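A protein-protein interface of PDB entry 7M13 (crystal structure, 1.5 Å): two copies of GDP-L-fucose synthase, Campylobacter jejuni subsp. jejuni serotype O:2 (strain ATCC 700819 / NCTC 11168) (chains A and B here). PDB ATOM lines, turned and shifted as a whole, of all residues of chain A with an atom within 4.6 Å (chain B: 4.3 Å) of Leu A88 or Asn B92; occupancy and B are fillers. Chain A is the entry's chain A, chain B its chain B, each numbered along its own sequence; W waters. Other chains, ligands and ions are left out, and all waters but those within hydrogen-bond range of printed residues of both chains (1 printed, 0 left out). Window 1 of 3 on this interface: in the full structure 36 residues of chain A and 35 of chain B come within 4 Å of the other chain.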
ATOM      1  N   ILE A  84     -22.964  15.411   8.296  1.00  0.00           N
ATOM      2  CA  ILE A  84     -21.615  15.158   8.847  1.00  0.00           C
ATOM      3  C   ILE A  84     -21.639  15.423  10.358  1.00  0.00           C
ATOM      4  O   ILE A  84     -21.139  14.589  11.123  1.00  0.00           O
ATOM      5  CB  ILE A  84     -20.514  15.868   8.048  1.00  0.00           C
ATOM      6  CG1 ILE A  84     -19.160  15.559   8.685  1.00  0.00           C
ATOM      7  CG2 ILE A  84     -20.690  17.355   7.867  1.00  0.00           C
ATOM      8  CD1 ILE A  84     -18.001  15.809   7.750  1.00  0.00           C
ATOM      9  N   TYR A  85     -22.167  16.539  10.827  1.00  0.00           N
ATOM     10  CA  TYR A  85     -22.102  16.855  12.270  1.00  0.00           C
ATOM     11  C   TYR A  85     -22.869  15.801  13.085  1.00  0.00           C
ATOM     12  O   TYR A  85     -22.347  15.271  14.066  1.00  0.00           O
ATOM     13  CB  TYR A  85     -22.631  18.253  12.555  1.00  0.00           C
ATOM     14  CG  TYR A  85     -22.760  18.501  14.030  1.00  0.00           C
ATOM     15  CD1 TYR A  85     -21.644  18.703  14.834  1.00  0.00           C
ATOM     16  CD2 TYR A  85     -23.992  18.509  14.637  1.00  0.00           C
ATOM     17  CE1 TYR A  85     -21.764  18.915  16.199  1.00  0.00           C
ATOM     18  CE2 TYR A  85     -24.130  18.727  16.002  1.00  0.00           C
ATOM     19  CZ  TYR A  85     -23.011  18.936  16.793  1.00  0.00           C
ATOM     20  OH  TYR A  85     -23.100  19.123  18.165  1.00  0.00           O
ATOM     21  N   GLU A  86     -24.142  15.560  12.759  1.00  0.00           N
ATOM     22  CA  GLU A  86     -24.974  14.710  13.638  1.00  0.00           C
ATOM     23  C   GLU A  86     -24.436  13.286  13.638  1.00  0.00           C
ATOM     24  O   GLU A  86     -24.345  12.677  14.715  1.00  0.00           O
ATOM     25  CB  GLU A  86     -26.416  14.768  13.214  1.00  0.00           C
ATOM     26  CG  GLU A  86     -26.996  16.137  13.501  1.00  0.00           C
ATOM     27  CD  GLU A  86     -28.493  16.249  13.323  1.00  0.00           C
ATOM     28  OE1 GLU A  86     -29.198  15.209  13.437  1.00  0.00           O
ATOM     29  OE2 GLU A  86     -28.937  17.376  13.023  1.00  0.00           O
ATOM     30  N   ASN A  87     -24.031  12.758  12.476  1.00  0.00           N
ATOM     31  CA  ASN A  87     -23.546  11.376  12.408  1.00  0.00           C
ATOM     32  C   ASN A  87     -22.175  11.286  13.091  1.00  0.00           C
ATOM     33  O   ASN A  87     -21.923  10.306  13.773  1.00  0.00           O
ATOM     34  CB  ASN A  87     -23.607  10.834  10.983  1.00  0.00           C
ATOM     35  CG  ASN A  87     -25.046  10.628  10.563  1.00  0.00           C
ATOM     36  OD1 ASN A  87     -25.812   9.998  11.305  1.00  0.00           O
ATOM     37  ND2 ASN A  87     -25.410  11.161   9.404  1.00  0.00           N
ATOM     38  N   LEU A  88     -21.298  12.277  12.918  1.00  0.00           N
ATOM     39  CA  LEU A  88     -19.995  12.191  13.645  1.00  0.00           C
ATOM     40  C   LEU A  88     -20.281  12.237  15.133  1.00  0.00           C
ATOM     41  O   LEU A  88     -19.616  11.515  15.869  1.00  0.00           O
ATOM     42  CB  LEU A  88     -19.101  13.366  13.264  1.00  0.00           C
ATOM     43  CG  LEU A  88     -18.422  13.320  11.891  1.00  0.00           C
ATOM     44  CD1 LEU A  88     -17.579  14.574  11.730  1.00  0.00           C
ATOM     45  CD2 LEU A  88     -17.590  12.072  11.707  1.00  0.00           C
ATOM     46  N   MET A  89     -21.228  13.043  15.595  1.00  0.00           N
ATOM     47  CA  MET A  89     -21.472  13.123  17.055  1.00  0.00           C
ATOM     48  C   MET A  89     -22.029  11.785  17.577  1.00  0.00           C
ATOM     49  O   MET A  89     -21.592  11.321  18.647  1.00  0.00           O
ATOM     50  CB  MET A  89     -22.433  14.267  17.393  1.00  0.00           C
ATOM     51  CG  MET A  89     -21.834  15.659  17.280  1.00  0.00           C
ATOM     52  SD  MET A  89     -20.296  15.928  18.133  1.00  0.00           S
ATOM     53  CE  MET A  89     -20.842  15.677  19.818  1.00  0.00           C
ATOM     54  N   ILE A  90     -23.009  11.218  16.898  1.00  0.00           N
ATOM     55  CA  ILE A  90     -23.584   9.896  17.287  1.00  0.00           C
ATOM     56  C   ILE A  90     -22.475   8.858  17.353  1.00  0.00           C
ATOM     57  O   ILE A  90     -22.296   8.151  18.354  1.00  0.00           O
ATOM     58  CB  ILE A  90     -24.700   9.461  16.358  1.00  0.00           C
ATOM     59  CG1 ILE A  90     -25.908  10.396  16.453  1.00  0.00           C
ATOM     60  CG2 ILE A  90     -25.041   7.995  16.591  1.00  0.00           C
ATOM     61  CD1 ILE A  90     -26.932  10.256  15.363  1.00  0.00           C
ATOM     62  N   GLN A  91     -21.733   8.746  16.274  1.00  0.00           N
ATOM     63  CA  GLN A  91     -20.597   7.811  16.192  1.00  0.00           C
ATOM     64  C   GLN A  91     -19.615   8.051  17.342  1.00  0.00           C
ATOM     65  O   GLN A  91     -19.215   7.104  18.036  1.00  0.00           O
ATOM     66  CB  GLN A  91     -19.920   7.983  14.826  1.00  0.00           C
ATOM     67  CG  GLN A  91     -20.732   7.494  13.657  1.00  0.00           C
ATOM     68  CD  GLN A  91     -20.248   7.959  12.300  1.00  0.00           C
ATOM     69  OE1 GLN A  91     -20.994   7.837  11.321  1.00  0.00           O
ATOM     70  NE2 GLN A  91     -19.050   8.528  12.235  1.00  0.00           N
ATOM     71  N   ASN A  92     -19.171   9.289  17.507  1.00  0.00           N
ATOM     72  CA  ASN A  92     -18.094   9.586  18.468  1.00  0.00           C
ATOM     73  C   ASN A  92     -18.630   9.319  19.876  1.00  0.00           C
ATOM     74  O   ASN A  92     -17.936   8.708  20.696  1.00  0.00           O
ATOM     75  CB  ASN A  92     -17.623  11.036  18.364  1.00  0.00           C
ATOM     76  CG  ASN A  92     -16.897  11.392  17.075  1.00  0.00           C
ATOM     77  OD1 ASN A  92     -16.691  12.612  16.839  1.00  0.00           O
ATOM     78  ND2 ASN A  92     -16.517  10.409  16.344  1.00  0.00           N
ATOM     79  N   ALA A 143     -18.584  11.159   6.859  1.00  0.00           N
ATOM     80  CA  ALA A 143     -18.894  10.798   8.261  1.00  0.00           C
ATOM     81  C   ALA A 143     -18.813   9.275   8.435  1.00  0.00           C
ATOM     82  O   ALA A 143     -18.204   8.822   9.440  1.00  0.00           O
ATOM     83  CB  ALA A 143     -20.236  11.348   8.648  1.00  0.00           C
ATOM     84  N   ALA A 146     -15.242   8.249   8.670  1.00  0.00           N
ATOM     85  CA  ALA A 146     -14.736   8.561  10.031  1.00  0.00           C
ATOM     86  C   ALA A 146     -15.224   7.526  11.055  1.00  0.00           C
ATOM     87  O   ALA A 146     -14.447   7.170  11.969  1.00  0.00           O
ATOM     88  CB  ALA A 146     -15.121   9.950  10.460  1.00  0.00           C
ATOM     89  N   LEU B  88     -11.734  15.194  16.155  1.00  0.00           N
ATOM     90  CA  LEU B  88     -13.149  15.337  15.710  1.00  0.00           C
ATOM     91  C   LEU B  88     -13.961  16.079  16.769  1.00  0.00           C
ATOM     92  O   LEU B  88     -14.802  16.895  16.410  1.00  0.00           O
ATOM     93  CB  LEU B  88     -13.780  13.972  15.398  1.00  0.00           C
ATOM     94  CG  LEU B  88     -13.294  13.257  14.152  1.00  0.00           C
ATOM     95  CD1 LEU B  88     -13.984  11.913  14.032  1.00  0.00           C
ATOM     96  CD2 LEU B  88     -13.512  14.082  12.895  1.00  0.00           C
ATOM     97  N   MET B  89     -13.798  15.771  18.059  1.00  0.00           N
ATOM     98  CA  MET B  89     -14.602  16.441  19.093  1.00  0.00           C
ATOM     99  C   MET B  89     -14.270  17.948  19.134  1.00  0.00           C
ATOM    100  O   MET B  89     -15.214  18.754  19.181  1.00  0.00           O
ATOM    101  CB  MET B  89     -14.441  15.829  20.478  1.00  0.00           C
ATOM    102  CG  MET B  89     -15.002  14.381  20.597  1.00  0.00           C
ATOM    103  SD  MET B  89     -16.763  14.268  20.240  1.00  0.00           S
ATOM    104  CE  MET B  89     -17.380  15.444  21.431  1.00  0.00           C
ATOM    105  N   ILE B  90     -13.005  18.308  19.107  1.00  0.00           N
ATOM    106  CA  ILE B  90     -12.603  19.732  19.124  1.00  0.00           C
ATOM    107  C   ILE B  90     -13.264  20.434  17.935  1.00  0.00           C
ATOM    108  O   ILE B  90     -13.889  21.487  18.072  1.00  0.00           O
ATOM    109  CB  ILE B  90     -11.081  19.865  19.139  1.00  0.00           C
ATOM    110  CG1 ILE B  90     -10.513  19.366  20.469  1.00  0.00           C
ATOM    111  CG2 ILE B  90     -10.720  21.322  18.879  1.00  0.00           C
ATOM    112  CD1 ILE B  90      -9.020  19.212  20.456  1.00  0.00           C
ATOM    113  N   GLN B  91     -13.041  19.883  16.757  1.00  0.00           N
ATOM    114  CA  GLN B  91     -13.553  20.447  15.494  1.00  0.00           C
ATOM    115  C   GLN B  91     -15.071  20.583  15.586  1.00  0.00           C
ATOM    116  O   GLN B  91     -15.639  21.686  15.294  1.00  0.00           O
ATOM    117  CB  GLN B  91     -13.166  19.577  14.296  1.00  0.00           C
ATOM    118  CG  GLN B  91     -11.668  19.559  14.002  1.00  0.00           C
ATOM    119  CD  GLN B  91     -11.190  18.424  13.134  1.00  0.00           C
ATOM    120  OE1 GLN B  91      -9.971  18.203  13.064  1.00  0.00           O
ATOM    121  NE2 GLN B  91     -12.095  17.659  12.554  1.00  0.00           N
ATOM    122  N   ASN B  92     -15.759  19.509  15.945  1.00  0.00           N
ATOM    123  CA  ASN B  92     -17.232  19.489  15.891  1.00  0.00           C
ATOM    124  C   ASN B  92     -17.767  20.467  16.943  1.00  0.00           C
ATOM    125  O   ASN B  92     -18.701  21.241  16.666  1.00  0.00           O
ATOM    126  CB  ASN B  92     -17.767  18.086  16.148  1.00  0.00           C
ATOM    127  CG  ASN B  92     -17.500  17.121  15.016  1.00  0.00           C
ATOM    128  OD1 ASN B  92     -17.044  17.515  13.957  1.00  0.00           O
ATOM    129  ND2 ASN B  92     -17.782  15.865  15.299  1.00  0.00           N
ATOM    130  N   ASN B  93     -17.201  20.429  18.137  1.00  0.00           N
ATOM    131  CA  ASN B  93     -17.713  21.300  19.220  1.00  0.00           C
ATOM    132  C   ASN B  93     -17.522  22.774  18.848  1.00  0.00           C
ATOM    133  O   ASN B  93     -18.467  23.564  19.004  1.00  0.00           O
ATOM    134  CB  ASN B  93     -17.012  20.980  20.529  1.00  0.00           C
ATOM    135  CG  ASN B  93     -17.399  19.644  21.145  1.00  0.00           C
ATOM    136  OD1 ASN B  93     -18.446  19.095  20.823  1.00  0.00           O
ATOM    137  ND2 ASN B  93     -16.534  19.161  22.022  1.00  0.00           N
ATOM    138  N   VAL B  94     -16.358  23.153  18.329  1.00  0.00           N
ATOM    139  CA  VAL B  94     -16.109  24.595  18.061  1.00  0.00           C
ATOM    140  C   VAL B  94     -16.883  25.017  16.812  1.00  0.00           C
ATOM    141  O   VAL B  94     -17.531  26.059  16.824  1.00  0.00           O
ATOM    142  CB  VAL B  94     -14.601  24.852  17.943  1.00  0.00           C
ATOM    143  CG1 VAL B  94     -14.298  26.240  17.431  1.00  0.00           C
ATOM    144  CG2 VAL B  94     -13.938  24.586  19.285  1.00  0.00           C
ATOM    145  N   ILE B  95     -16.899  24.202  15.763  1.00  0.00           N
ATOM    146  CA  ILE B  95     -17.550  24.618  14.505  1.00  0.00           C
ATOM    147  C   ILE B  95     -19.068  24.697  14.735  1.00  0.00           C
ATOM    148  O   ILE B  95     -19.708  25.693  14.372  1.00  0.00           O
ATOM    149  CB  ILE B  95     -17.176  23.699  13.340  1.00  0.00           C
ATOM    150  CG1 ILE B  95     -15.700  23.846  12.994  1.00  0.00           C
ATOM    151  CG2 ILE B  95     -18.066  24.006  12.148  1.00  0.00           C
ATOM    152  CD1 ILE B  95     -15.172  22.741  12.103  1.00  0.00           C
ATOM    153  N   HIS B  96     -19.673  23.666  15.330  1.00  0.00           N
ATOM    154  CA  HIS B  96     -21.138  23.666  15.500  1.00  0.00           C
ATOM    155  C   HIS B  96     -21.555  24.789  16.463  1.00  0.00           C
ATOM    156  O   HIS B  96     -22.565  25.450  16.175  1.00  0.00           O
ATOM    157  CB  HIS B  96     -21.643  22.302  15.981  1.00  0.00           C
ATOM    158  CG  HIS B  96     -23.113  22.275  16.103  1.00  0.00           C
ATOM    159  ND1 HIS B  96     -23.881  22.267  14.985  1.00  0.00           N
ATOM    160  CD2 HIS B  96     -23.947  22.274  17.169  1.00  0.00           C
ATOM    161  CE1 HIS B  96     -25.162  22.251  15.347  1.00  0.00           C
ATOM    162  NE2 HIS B  96     -25.229  22.246  16.672  1.00  0.00           N
ATOM    163  N   ALA B 146     -12.359  15.550   7.806  1.00  0.00           N
ATOM    164  CA  ALA B 146     -13.725  15.768   8.321  1.00  0.00           C
ATOM    165  C   ALA B 146     -13.852  17.225   8.782  1.00  0.00           C
ATOM    166  O   ALA B 146     -14.935  17.800   8.649  1.00  0.00           O
ATOM    167  CB  ALA B 146     -14.022  14.838   9.468  1.00  0.00           C
ATOM    168  N   MET B 150     -16.531  19.643   7.239  1.00  0.00           N
ATOM    169  CA  MET B 150     -17.461  20.242   8.233  1.00  0.00           C
ATOM    170  C   MET B 150     -17.601  21.743   7.948  1.00  0.00           C
ATOM    171  O   MET B 150     -18.743  22.241   7.977  1.00  0.00           O
ATOM    172  CB  MET B 150     -16.939  20.042   9.660  1.00  0.00           C
ATOM    173  CG  MET B 150     -17.434  18.764  10.309  1.00  0.00           C
ATOM    174  SD  MET B 150     -19.081  18.951  11.041  1.00  0.00           S
ATOM    175  CE  MET B 150     -18.713  20.054  12.404  1.00  0.00           C
HETATM  176  O   HOH W   1     -21.108  20.157  19.826  1.00  0.00           O
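The side-chain amide nitrogen of Asn B92 lies within hydrogen-bond range of the side-chain sulfur of Met A89, 3.8 Å away.
SD of Met B89 lies close to OD1 of Asn A92 (3.8 Å).
Hydrophobic or aromatic side chains of chain B within 4 Å of the printed part of chain A: Leu B88, Met B89, His B96 and Met B150.
Among the printed residues, 11 pairs touch across the chains.
Among the printed residues, no Asp or Glu carboxylate lies within 4 Å of a Lys or Arg side-chain nitrogen of the other chain.
Of chain B, only Asn B92 (3.5 Å) comes within 4 Å of Leu A88.
Printed residues of chain B within 4 Å of Met A89: Met B89 and Asn B92.
Printed residues of chain A within 4 Å of Leu B88: Asn A92 (3.5 Å).
Printed residues of chain A within 4 Å of Asn B92: Tyr A85, Leu A88, Met A89 and Asn A92.
Of the printed residues of chain A, His B96 touches Tyr A85.
The nearest residue of chain B that does not touch Leu A88 is Ala B146 (4.2 Å).
The nearest printed residue of chain A that does not touch Asn B92 is Ile A84 (5.5 Å).
The nearest printed residue of chain A that does not touch Met B150 is Leu A88 (4.4 Å).
Water W1 bridges the side-chain hydroxyl of Tyr A85 (2.8 Å) and the side-chain amide oxygen of Asn B93 (3.0 Å).
Leu A88 touches Asn B92, and with the chains exchanged Asn A92 touches Leu B88.
Met B89 touches its own counterpart, Met A89.
Met A89 touches Asn B92, and with the chains exchanged Asn A92 touches Met B89.
Asn A92 touches its own counterpart, Asn B92.
Positions printed for both chains: 88, 89, 90, 91, 92 and 146.
Of the 11 pairs that touch across the chains among the printed residues, 6 have their exchanged pair printed and touching as well.
Among the printed residues, pairs that only touch across the chains: Ile A84 with Ala B146 (3.8 Å), Ile A84 with Met B150 (3.9 Å), Tyr A85 with Asn B92 (3.9 Å), Tyr A85 with His B96 (3.4 Å), Tyr A85 with Met B150 (3.9 Å), Leu A88 with Asn B92 (3.5 Å), Met A89 with Met B89 (3.8 Å), Asn A92 with Leu B88 (3.5 Å) and Asn A92 with Asn B92 (3.8 Å).
The side-chain amide oxygen (OD1) of Asn A92 sits close to the backbone carbonyl oxygen (O) of Leu A88 (3.3 Å).
The side-chain amide nitrogen of Asn B92 sits close to the backbone carbonyl oxygen of Leu B88, 3.3 Å away.
The backbone carbonyl oxygen (O) of Met B89 sits close to the side-chain amide nitrogen (ND2) of Asn B93 (3.2 Å).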
